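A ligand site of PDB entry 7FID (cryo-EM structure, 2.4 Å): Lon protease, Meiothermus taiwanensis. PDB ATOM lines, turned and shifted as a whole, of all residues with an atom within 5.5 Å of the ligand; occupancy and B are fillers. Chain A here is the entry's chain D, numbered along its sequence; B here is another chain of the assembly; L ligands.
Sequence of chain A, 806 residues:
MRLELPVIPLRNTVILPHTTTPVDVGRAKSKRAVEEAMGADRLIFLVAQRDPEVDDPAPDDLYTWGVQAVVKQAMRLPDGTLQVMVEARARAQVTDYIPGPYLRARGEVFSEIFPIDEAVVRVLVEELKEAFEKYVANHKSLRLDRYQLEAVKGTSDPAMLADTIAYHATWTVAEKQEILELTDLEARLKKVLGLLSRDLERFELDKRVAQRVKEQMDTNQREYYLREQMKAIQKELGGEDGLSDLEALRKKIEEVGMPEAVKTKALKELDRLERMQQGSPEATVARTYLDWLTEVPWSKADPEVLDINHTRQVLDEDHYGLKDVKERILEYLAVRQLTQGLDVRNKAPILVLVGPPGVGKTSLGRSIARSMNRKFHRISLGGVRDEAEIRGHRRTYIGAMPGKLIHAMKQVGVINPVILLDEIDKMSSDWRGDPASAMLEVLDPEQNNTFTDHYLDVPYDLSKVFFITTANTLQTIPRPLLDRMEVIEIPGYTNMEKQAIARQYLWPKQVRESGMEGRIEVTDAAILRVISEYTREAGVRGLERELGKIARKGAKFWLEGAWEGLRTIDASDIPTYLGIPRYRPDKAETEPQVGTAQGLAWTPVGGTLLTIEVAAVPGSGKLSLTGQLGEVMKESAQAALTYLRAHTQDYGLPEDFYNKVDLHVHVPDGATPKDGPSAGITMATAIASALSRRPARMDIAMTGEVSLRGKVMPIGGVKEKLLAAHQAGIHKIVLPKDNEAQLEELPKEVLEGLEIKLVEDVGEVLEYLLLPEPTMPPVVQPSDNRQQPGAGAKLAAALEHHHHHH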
ATOM      1  N   ASP A 318     -23.893  10.157  18.909  1.00  0.00           N
ATOM      2  CA  ASP A 318     -24.642  11.188  19.590  1.00  0.00           C
ATOM      3  C   ASP A 318     -25.112  10.746  20.965  1.00  0.00           C
ATOM      4  O   ASP A 318     -25.523  11.588  21.767  1.00  0.00           O
ATOM      5  CB  ASP A 318     -25.854  11.603  18.730  1.00  0.00           C
ATOM      6  CG  ASP A 318     -26.353  12.996  19.051  1.00  0.00           C
ATOM      7  OD1 ASP A 318     -25.754  13.683  19.898  1.00  0.00           O
ATOM      8  OD2 ASP A 318     -27.358  13.412  18.435  1.00  0.00           O
ATOM      9  N   HIS A 319     -25.040   9.456  21.271  1.00  0.00           N
ATOM     10  CA  HIS A 319     -25.361   8.970  22.596  1.00  0.00           C
ATOM     11  C   HIS A 319     -24.438   7.814  22.929  1.00  0.00           C
ATOM     12  O   HIS A 319     -23.844   7.186  22.055  1.00  0.00           O
ATOM     13  CB  HIS A 319     -26.823   8.535  22.698  1.00  0.00           C
ATOM     14  CG  HIS A 319     -27.794   9.667  22.721  1.00  0.00           C
ATOM     15  ND1 HIS A 319     -28.287  10.251  21.579  1.00  0.00           N
ATOM     16  CD2 HIS A 319     -28.382  10.311  23.750  1.00  0.00           C
ATOM     17  CE1 HIS A 319     -29.123  11.215  21.905  1.00  0.00           C
ATOM     18  NE2 HIS A 319     -29.200  11.270  23.226  1.00  0.00           N
ATOM     19  N   TYR A 320     -24.325   7.541  24.222  1.00  0.00           N
ATOM     20  CA  TYR A 320     -23.491   6.499  24.770  1.00  0.00           C
ATOM     21  C   TYR A 320     -24.380   5.448  25.400  1.00  0.00           C
ATOM     22  O   TYR A 320     -25.319   5.781  26.122  1.00  0.00           O
ATOM     23  CB  TYR A 320     -22.555   7.071  25.835  1.00  0.00           C
ATOM     24  CG  TYR A 320     -21.629   6.065  26.440  1.00  0.00           C
ATOM     25  CD1 TYR A 320     -20.504   5.649  25.761  1.00  0.00           C
ATOM     26  CD2 TYR A 320     -21.857   5.539  27.701  1.00  0.00           C
ATOM     27  CE1 TYR A 320     -19.646   4.736  26.308  1.00  0.00           C
ATOM     28  CE2 TYR A 320     -21.005   4.624  28.256  1.00  0.00           C
ATOM     29  CZ  TYR A 320     -19.904   4.227  27.550  1.00  0.00           C
ATOM     30  OH  TYR A 320     -19.039   3.309  28.102  1.00  0.00           O
ATOM     31  N   GLY A 321     -24.087   4.176  25.125  1.00  0.00           N
ATOM     32  CA  GLY A 321     -24.909   3.110  25.652  1.00  0.00           C
ATOM     33  C   GLY A 321     -26.284   3.106  25.019  1.00  0.00           C
ATOM     34  O   GLY A 321     -26.419   3.266  23.804  1.00  0.00           O
ATOM     35  N   LEU A 322     -27.300   2.929  25.868  1.00  0.00           N
ATOM     36  CA  LEU A 322     -28.714   2.896  25.486  1.00  0.00           C
ATOM     37  C   LEU A 322     -28.987   1.845  24.417  1.00  0.00           C
ATOM     38  O   LEU A 322     -29.372   2.145  23.295  1.00  0.00           O
ATOM     39  CB  LEU A 322     -29.205   4.271  25.022  1.00  0.00           C
ATOM     40  CG  LEU A 322     -29.200   5.359  26.092  1.00  0.00           C
ATOM     41  CD1 LEU A 322     -29.625   6.669  25.479  1.00  0.00           C
ATOM     42  CD2 LEU A 322     -30.096   4.970  27.226  1.00  0.00           C
ATOM     43  N   PRO A 356     -36.090   7.929  34.375  1.00  0.00           N
ATOM     44  CA  PRO A 356     -35.945   9.072  35.270  1.00  0.00           C
ATOM     45  C   PRO A 356     -35.552  10.309  34.493  1.00  0.00           C
ATOM     46  O   PRO A 356     -35.082  10.194  33.352  1.00  0.00           O
ATOM     47  CB  PRO A 356     -34.821   8.611  36.208  1.00  0.00           C
ATOM     48  CG  PRO A 356     -34.049   7.675  35.411  1.00  0.00           C
ATOM     49  CD  PRO A 356     -35.014   6.953  34.548  1.00  0.00           C
ATOM     50  N   PRO A 357     -35.748  11.509  35.033  1.00  0.00           N
ATOM     51  CA  PRO A 357     -35.428  12.708  34.274  1.00  0.00           C
ATOM     52  C   PRO A 357     -33.935  12.928  34.148  1.00  0.00           C
ATOM     53  O   PRO A 357     -33.145  12.479  34.978  1.00  0.00           O
ATOM     54  CB  PRO A 357     -36.074  13.830  35.090  1.00  0.00           C
ATOM     55  CG  PRO A 357     -36.133  13.309  36.445  1.00  0.00           C
ATOM     56  CD  PRO A 357     -36.387  11.850  36.325  1.00  0.00           C
ATOM     57  N   GLY A 358     -33.557  13.619  33.080  1.00  0.00           N
ATOM     58  CA  GLY A 358     -32.171  13.887  32.813  1.00  0.00           C
ATOM     59  C   GLY A 358     -31.478  12.861  31.971  1.00  0.00           C
ATOM     60  O   GLY A 358     -30.369  13.102  31.506  1.00  0.00           O
ATOM     61  N   VAL A 359     -32.085  11.708  31.761  1.00  0.00           N
ATOM     62  CA  VAL A 359     -31.569  10.755  30.806  1.00  0.00           C
ATOM     63  C   VAL A 359     -32.015  11.183  29.414  1.00  0.00           C
ATOM     64  O   VAL A 359     -32.996  11.900  29.243  1.00  0.00           O
ATOM     65  CB  VAL A 359     -32.060   9.345  31.166  1.00  0.00           C
ATOM     66  CG1 VAL A 359     -31.265   8.305  30.467  1.00  0.00           C
ATOM     67  CG2 VAL A 359     -31.977   9.122  32.643  1.00  0.00           C
ATOM     68  N   GLY A 360     -31.288  10.760  28.393  1.00  0.00           N
ATOM     69  CA  GLY A 360     -31.503  11.296  27.069  1.00  0.00           C
ATOM     70  C   GLY A 360     -32.737  10.789  26.384  1.00  0.00           C
ATOM     71  O   GLY A 360     -32.634   9.921  25.521  1.00  0.00           O
ATOM     72  N   LYS A 361     -33.926  11.270  26.757  1.00  0.00           N
ATOM     73  CA  LYS A 361     -35.135  10.832  26.075  1.00  0.00           C
ATOM     74  C   LYS A 361     -35.483  11.723  24.885  1.00  0.00           C
ATOM     75  O   LYS A 361     -35.777  11.218  23.800  1.00  0.00           O
ATOM     76  CB  LYS A 361     -36.302  10.758  27.054  1.00  0.00           C
ATOM     77  CG  LYS A 361     -36.155   9.689  28.100  1.00  0.00           C
ATOM     78  CD  LYS A 361     -37.445   9.439  28.831  1.00  0.00           C
ATOM     79  CE  LYS A 361     -37.823  10.523  29.793  1.00  0.00           C
ATOM     80  NZ  LYS A 361     -36.950  10.528  30.972  1.00  0.00           N
ATOM     81  N   THR A 362     -35.440  13.049  25.070  1.00  0.00           N
ATOM     82  CA  THR A 362     -35.815  13.963  23.989  1.00  0.00           C
ATOM     83  C   THR A 362     -34.731  14.016  22.910  1.00  0.00           C
ATOM     84  O   THR A 362     -35.020  13.944  21.699  1.00  0.00           O
ATOM     85  CB  THR A 362     -36.042  15.344  24.584  1.00  0.00           C
ATOM     86  OG1 THR A 362     -37.053  15.258  25.598  1.00  0.00           O
ATOM     87  CG2 THR A 362     -36.495  16.308  23.530  1.00  0.00           C
ATOM     88  N   SER A 363     -33.474  14.134  23.330  1.00  0.00           N
ATOM     89  CA  SER A 363     -32.358  14.195  22.399  1.00  0.00           C
ATOM     90  C   SER A 363     -32.208  12.901  21.627  1.00  0.00           C
ATOM     91  O   SER A 363     -31.712  12.907  20.498  1.00  0.00           O
ATOM     92  CB  SER A 363     -31.094  14.524  23.164  1.00  0.00           C
ATOM     93  OG  SER A 363     -30.806  13.525  24.111  1.00  0.00           O
ATOM     94  N   LEU A 364     -32.667  11.789  22.204  1.00  0.00           N
ATOM     95  CA  LEU A 364     -32.678  10.539  21.461  1.00  0.00           C
ATOM     96  C   LEU A 364     -33.708  10.583  20.351  1.00  0.00           C
ATOM     97  O   LEU A 364     -33.494   9.999  19.303  1.00  0.00           O
ATOM     98  CB  LEU A 364     -32.948   9.387  22.399  1.00  0.00           C
ATOM     99  CG  LEU A 364     -32.775   7.968  21.919  1.00  0.00           C
ATOM    100  CD1 LEU A 364     -31.373   7.760  21.442  1.00  0.00           C
ATOM    101  CD2 LEU A 364     -33.030   7.074  23.104  1.00  0.00           C
ATOM    102  N   TYR A 493     -27.811   5.761  35.095  1.00  0.00           N
ATOM    103  CA  TYR A 493     -26.400   5.558  34.823  1.00  0.00           C
ATOM    104  C   TYR A 493     -25.592   5.286  36.074  1.00  0.00           C
ATOM    105  O   TYR A 493     -25.841   5.867  37.134  1.00  0.00           O
ATOM    106  CB  TYR A 493     -25.799   6.758  34.100  1.00  0.00           C
ATOM    107  CG  TYR A 493     -26.407   6.964  32.757  1.00  0.00           C
ATOM    108  CD1 TYR A 493     -26.079   6.134  31.714  1.00  0.00           C
ATOM    109  CD2 TYR A 493     -27.304   7.989  32.533  1.00  0.00           C
ATOM    110  CE1 TYR A 493     -26.645   6.303  30.481  1.00  0.00           C
ATOM    111  CE2 TYR A 493     -27.856   8.171  31.312  1.00  0.00           C
ATOM    112  CZ  TYR A 493     -27.524   7.329  30.294  1.00  0.00           C
ATOM    113  OH  TYR A 493     -28.082   7.494  29.066  1.00  0.00           O
ATOM    114  N   ILE A 501     -19.498   9.486  29.646  1.00  0.00           N
ATOM    115  CA  ILE A 501     -20.316  10.500  28.983  1.00  0.00           C
ATOM    116  C   ILE A 501     -19.712  11.876  29.176  1.00  0.00           C
ATOM    117  O   ILE A 501     -19.660  12.684  28.242  1.00  0.00           O
ATOM    118  CB  ILE A 501     -21.762  10.443  29.511  1.00  0.00           C
ATOM    119  CG1 ILE A 501     -22.444   9.152  29.116  1.00  0.00           C
ATOM    120  CG2 ILE A 501     -22.581  11.582  28.990  1.00  0.00           C
ATOM    121  CD1 ILE A 501     -23.734   8.939  29.840  1.00  0.00           C
ATOM    122  N   TYR A 505     -18.686  13.198  25.508  1.00  0.00           N
ATOM    123  CA  TYR A 505     -19.780  13.928  24.890  1.00  0.00           C
ATOM    124  C   TYR A 505     -20.038  15.293  25.499  1.00  0.00           C
ATOM    125  O   TYR A 505     -20.228  16.253  24.763  1.00  0.00           O
ATOM    126  CB  TYR A 505     -21.066  13.101  24.968  1.00  0.00           C
ATOM    127  CG  TYR A 505     -21.021  11.847  24.129  1.00  0.00           C
ATOM    128  CD1 TYR A 505     -21.252  11.894  22.767  1.00  0.00           C
ATOM    129  CD2 TYR A 505     -20.751  10.617  24.707  1.00  0.00           C
ATOM    130  CE1 TYR A 505     -21.203  10.754  22.009  1.00  0.00           C
ATOM    131  CE2 TYR A 505     -20.707   9.475  23.957  1.00  0.00           C
ATOM    132  CZ  TYR A 505     -20.943   9.552  22.609  1.00  0.00           C
ATOM    133  OH  TYR A 505     -20.892   8.405  21.864  1.00  0.00           O
ATOM    134  N   LEU A 506     -20.053  15.413  26.824  1.00  0.00           N
ATOM    135  CA  LEU A 506     -20.512  16.650  27.444  1.00  0.00           C
ATOM    136  C   LEU A 506     -19.449  17.737  27.423  1.00  0.00           C
ATOM    137  O   LEU A 506     -19.711  18.854  26.981  1.00  0.00           O
ATOM    138  CB  LEU A 506     -20.956  16.380  28.877  1.00  0.00           C
ATOM    139  CG  LEU A 506     -22.192  15.512  28.984  1.00  0.00           C
ATOM    140  CD1 LEU A 506     -22.501  15.205  30.419  1.00  0.00           C
ATOM    141  CD2 LEU A 506     -23.353  16.226  28.353  1.00  0.00           C
ATOM    142  N   LYS A 509     -18.475  19.460  24.014  1.00  0.00           N
ATOM    143  CA  LYS A 509     -19.565  20.320  23.579  1.00  0.00           C
ATOM    144  C   LYS A 509     -19.601  21.604  24.392  1.00  0.00           C
ATOM    145  O   LYS A 509     -19.798  22.689  23.831  1.00  0.00           O
ATOM    146  CB  LYS A 509     -20.877  19.568  23.688  1.00  0.00           C
ATOM    147  CG  LYS A 509     -22.073  20.364  23.279  1.00  0.00           C
ATOM    148  CD  LYS A 509     -23.305  19.487  23.264  1.00  0.00           C
ATOM    149  CE  LYS A 509     -23.746  19.139  24.662  1.00  0.00           C
ATOM    150  NZ  LYS A 509     -25.005  18.359  24.655  1.00  0.00           N
ATOM    151  N   VAL A 540     -27.962  13.139  33.730  1.00  0.00           N
ATOM    152  CA  VAL A 540     -26.721  13.884  33.558  1.00  0.00           C
ATOM    153  C   VAL A 540     -26.968  15.332  33.153  1.00  0.00           C
ATOM    154  O   VAL A 540     -26.068  15.955  32.563  1.00  0.00           O
ATOM    155  CB  VAL A 540     -25.794  13.214  32.528  1.00  0.00           C
ATOM    156  CG1 VAL A 540     -25.222  11.939  33.065  1.00  0.00           C
ATOM    157  CG2 VAL A 540     -26.561  12.953  31.273  1.00  0.00           C
ATOM    158  N   ARG A 541     -28.133  15.904  33.446  1.00  0.00           N
ATOM    159  CA  ARG A 541     -28.320  17.300  33.063  1.00  0.00           C
ATOM    160  C   ARG A 541     -27.620  18.226  34.042  1.00  0.00           C
ATOM    161  O   ARG A 541     -27.126  19.306  33.657  1.00  0.00           O
ATOM    162  CB  ARG A 541     -29.804  17.647  32.950  1.00  0.00           C
ATOM    163  CG  ARG A 541     -30.602  17.633  34.223  1.00  0.00           C
ATOM    164  CD  ARG A 541     -31.965  18.271  34.042  1.00  0.00           C
ATOM    165  NE  ARG A 541     -32.821  17.535  33.118  1.00  0.00           N
ATOM    166  CZ  ARG A 541     -33.145  17.961  31.910  1.00  0.00           C
ATOM    167  NH1 ARG A 541     -32.682  19.114  31.453  1.00  0.00           N
ATOM    168  NH2 ARG A 541     -33.940  17.221  31.140  1.00  0.00           N
ATOM    169  N   GLU A 544     -23.975  18.294  33.125  1.00  0.00           N
ATOM    170  CA  GLU A 544     -23.856  19.159  31.963  1.00  0.00           C
ATOM    171  C   GLU A 544     -23.802  20.626  32.352  1.00  0.00           C
ATOM    172  O   GLU A 544     -22.969  21.376  31.845  1.00  0.00           O
ATOM    173  CB  GLU A 544     -25.042  18.925  31.033  1.00  0.00           C
ATOM    174  CG  GLU A 544     -24.947  19.697  29.754  1.00  0.00           C
ATOM    175  CD  GLU A 544     -26.173  19.546  28.908  1.00  0.00           C
ATOM    176  OE1 GLU A 544     -27.140  18.905  29.374  1.00  0.00           O
ATOM    177  OE2 GLU A 544     -26.184  20.054  27.760  1.00  0.00           O
ATOM    178  N   ASP B 483     -36.024  24.204  29.847  1.00  0.00           N
ATOM    179  CA  ASP B 483     -34.918  23.413  29.330  1.00  0.00           C
ATOM    180  C   ASP B 483     -33.879  24.293  28.656  1.00  0.00           C
ATOM    181  O   ASP B 483     -32.703  23.921  28.561  1.00  0.00           O
ATOM    182  CB  ASP B 483     -35.430  22.348  28.363  1.00  0.00           C
ATOM    183  CG  ASP B 483     -36.152  21.219  29.073  1.00  0.00           C
ATOM    184  OD1 ASP B 483     -35.829  20.955  30.244  1.00  0.00           O
ATOM    185  OD2 ASP B 483     -37.022  20.571  28.449  1.00  0.00           O
HETATM  186  P1  LIG L   1     -35.029  14.360  29.564  1.00  0.00           P
HETATM  187  O1  LIG L   1     -35.809  15.648  29.598  1.00  0.00           O
HETATM  188  O2  LIG L   1     -35.256  13.550  28.331  1.00  0.00           O
HETATM  189  O3  LIG L   1     -35.057  13.588  30.840  1.00  0.00           O
HETATM  190  P2  LIG L   1     -32.942  15.359  28.018  1.00  0.00           P
HETATM  191  O4  LIG L   1     -33.805  16.535  27.668  1.00  0.00           O
HETATM  192  O5  LIG L   1     -32.814  14.255  27.014  1.00  0.00           O
HETATM  193  O6  LIG L   1     -33.480  14.775  29.409  1.00  0.00           O
HETATM  194  O7  LIG L   1     -31.476  15.921  28.333  1.00  0.00           O
HETATM  195  C1  LIG L   1     -30.418  15.100  28.813  1.00  0.00           C
HETATM  196  C2  LIG L   1     -29.096  15.682  28.353  1.00  0.00           C
HETATM  197  O8  LIG L   1     -28.055  14.718  28.442  1.00  0.00           O
HETATM  198  C3  LIG L   1     -29.198  16.050  26.898  1.00  0.00           C
HETATM  199  O9  LIG L   1     -28.848  17.425  26.777  1.00  0.00           O
HETATM  200  C4  LIG L   1     -28.175  15.236  26.172  1.00  0.00           C
HETATM  201  O10 LIG L   1     -27.445  16.076  25.275  1.00  0.00           O
HETATM  202  C5  LIG L   1     -27.249  14.781  27.268  1.00  0.00           C
HETATM  203  N1  LIG L   1     -26.598  13.496  26.911  1.00  0.00           N
HETATM  204  C6  LIG L   1     -25.547  13.357  26.087  1.00  0.00           C
HETATM  205  N2  LIG L   1     -25.166  12.075  25.959  1.00  0.00           N
HETATM  206  C7  LIG L   1     -25.996  11.370  26.721  1.00  0.00           C
HETATM  207  C8  LIG L   1     -26.164   9.962  27.050  1.00  0.00           C
HETATM  208  N3  LIG L   1     -25.349   9.041  26.519  1.00  0.00           N
HETATM  209  N4  LIG L   1     -27.149   9.622  27.882  1.00  0.00           N
HETATM  210  C9  LIG L   1     -27.957  10.539  28.418  1.00  0.00           C
HETATM  211  N5  LIG L   1     -27.869  11.843  28.164  1.00  0.00           N
HETATM  212  C10 LIG L   1     -26.929  12.296  27.343  1.00  0.00           C
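The backbone carbonyl oxygen (O) of Gly 358 is in hydrogen-bond range of the backbone NH (N) of Val 540, at 3.3 Å. The side-chain carboxylate (OD1) of Asp 483 of chain B lies within salt-bridge range of the guanidinium group (NH1) of Arg 541, at 3.8 Å. NZ of Lys 361 sits at hydrogen-bond distance from O of Pro 356. OE2 of Glu 544 lies within salt-bridge range of NZ of Lys 509, at 3.7 Å. The side-chain hydroxyl (OG) of Ser 363 is in hydrogen-bond range of a ring nitrogen (NE2) of His 319. O of Ile 501 sits at hydrogen-bond distance from N of Leu 506 (3.1 Å). The backbone carbonyl oxygen (O) of His 319 sits at hydrogen-bond distance from the side-chain hydroxyl (OH) of Tyr 505.
Merely in contact with the ligand: Gly 360, Val 540, Pro 357, Ser 363, Ile 501 and His 319. Of the 23 residues printed, 15 come within 4 Å of the ligand.
OH of Tyr 493 lies within hydrogen-bond range of N4 of the ligand, at 2.6 Å. The backbone NH (N) of Gly 358 is in hydrogen-bond range of an oxygen (O3) of the ligand. The guanidinium group (NH2) of Arg 541 lies within salt-bridge range of an oxygen (O1) of the ligand, 2.9 Å away. The backbone carbonyl oxygen (O) of Val 359 lies close to an oxygen (O2) of the ligand (2.9 Å). N3 of the ligand is in hydrogen-bond range of O of Tyr 320 (3.3 Å). N of Lys 361 is in hydrogen-bond range of O2 of the ligand (3.1 Å). An oxygen (O3) of the ligand is in salt-bridge range of the side-chain amino group (NZ) of Lys 361, 3.6 Å away. An oxygen (O2) of the ligand is in hydrogen-bond range of the backbone NH (N) of Thr 362 (3.3 Å). NZ of Lys 509 sits at hydrogen-bond distance from O10 of the ligand. An oxygen (O9) of the ligand is in hydrogen-bond range of the side-chain carboxylate of Glu 544.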
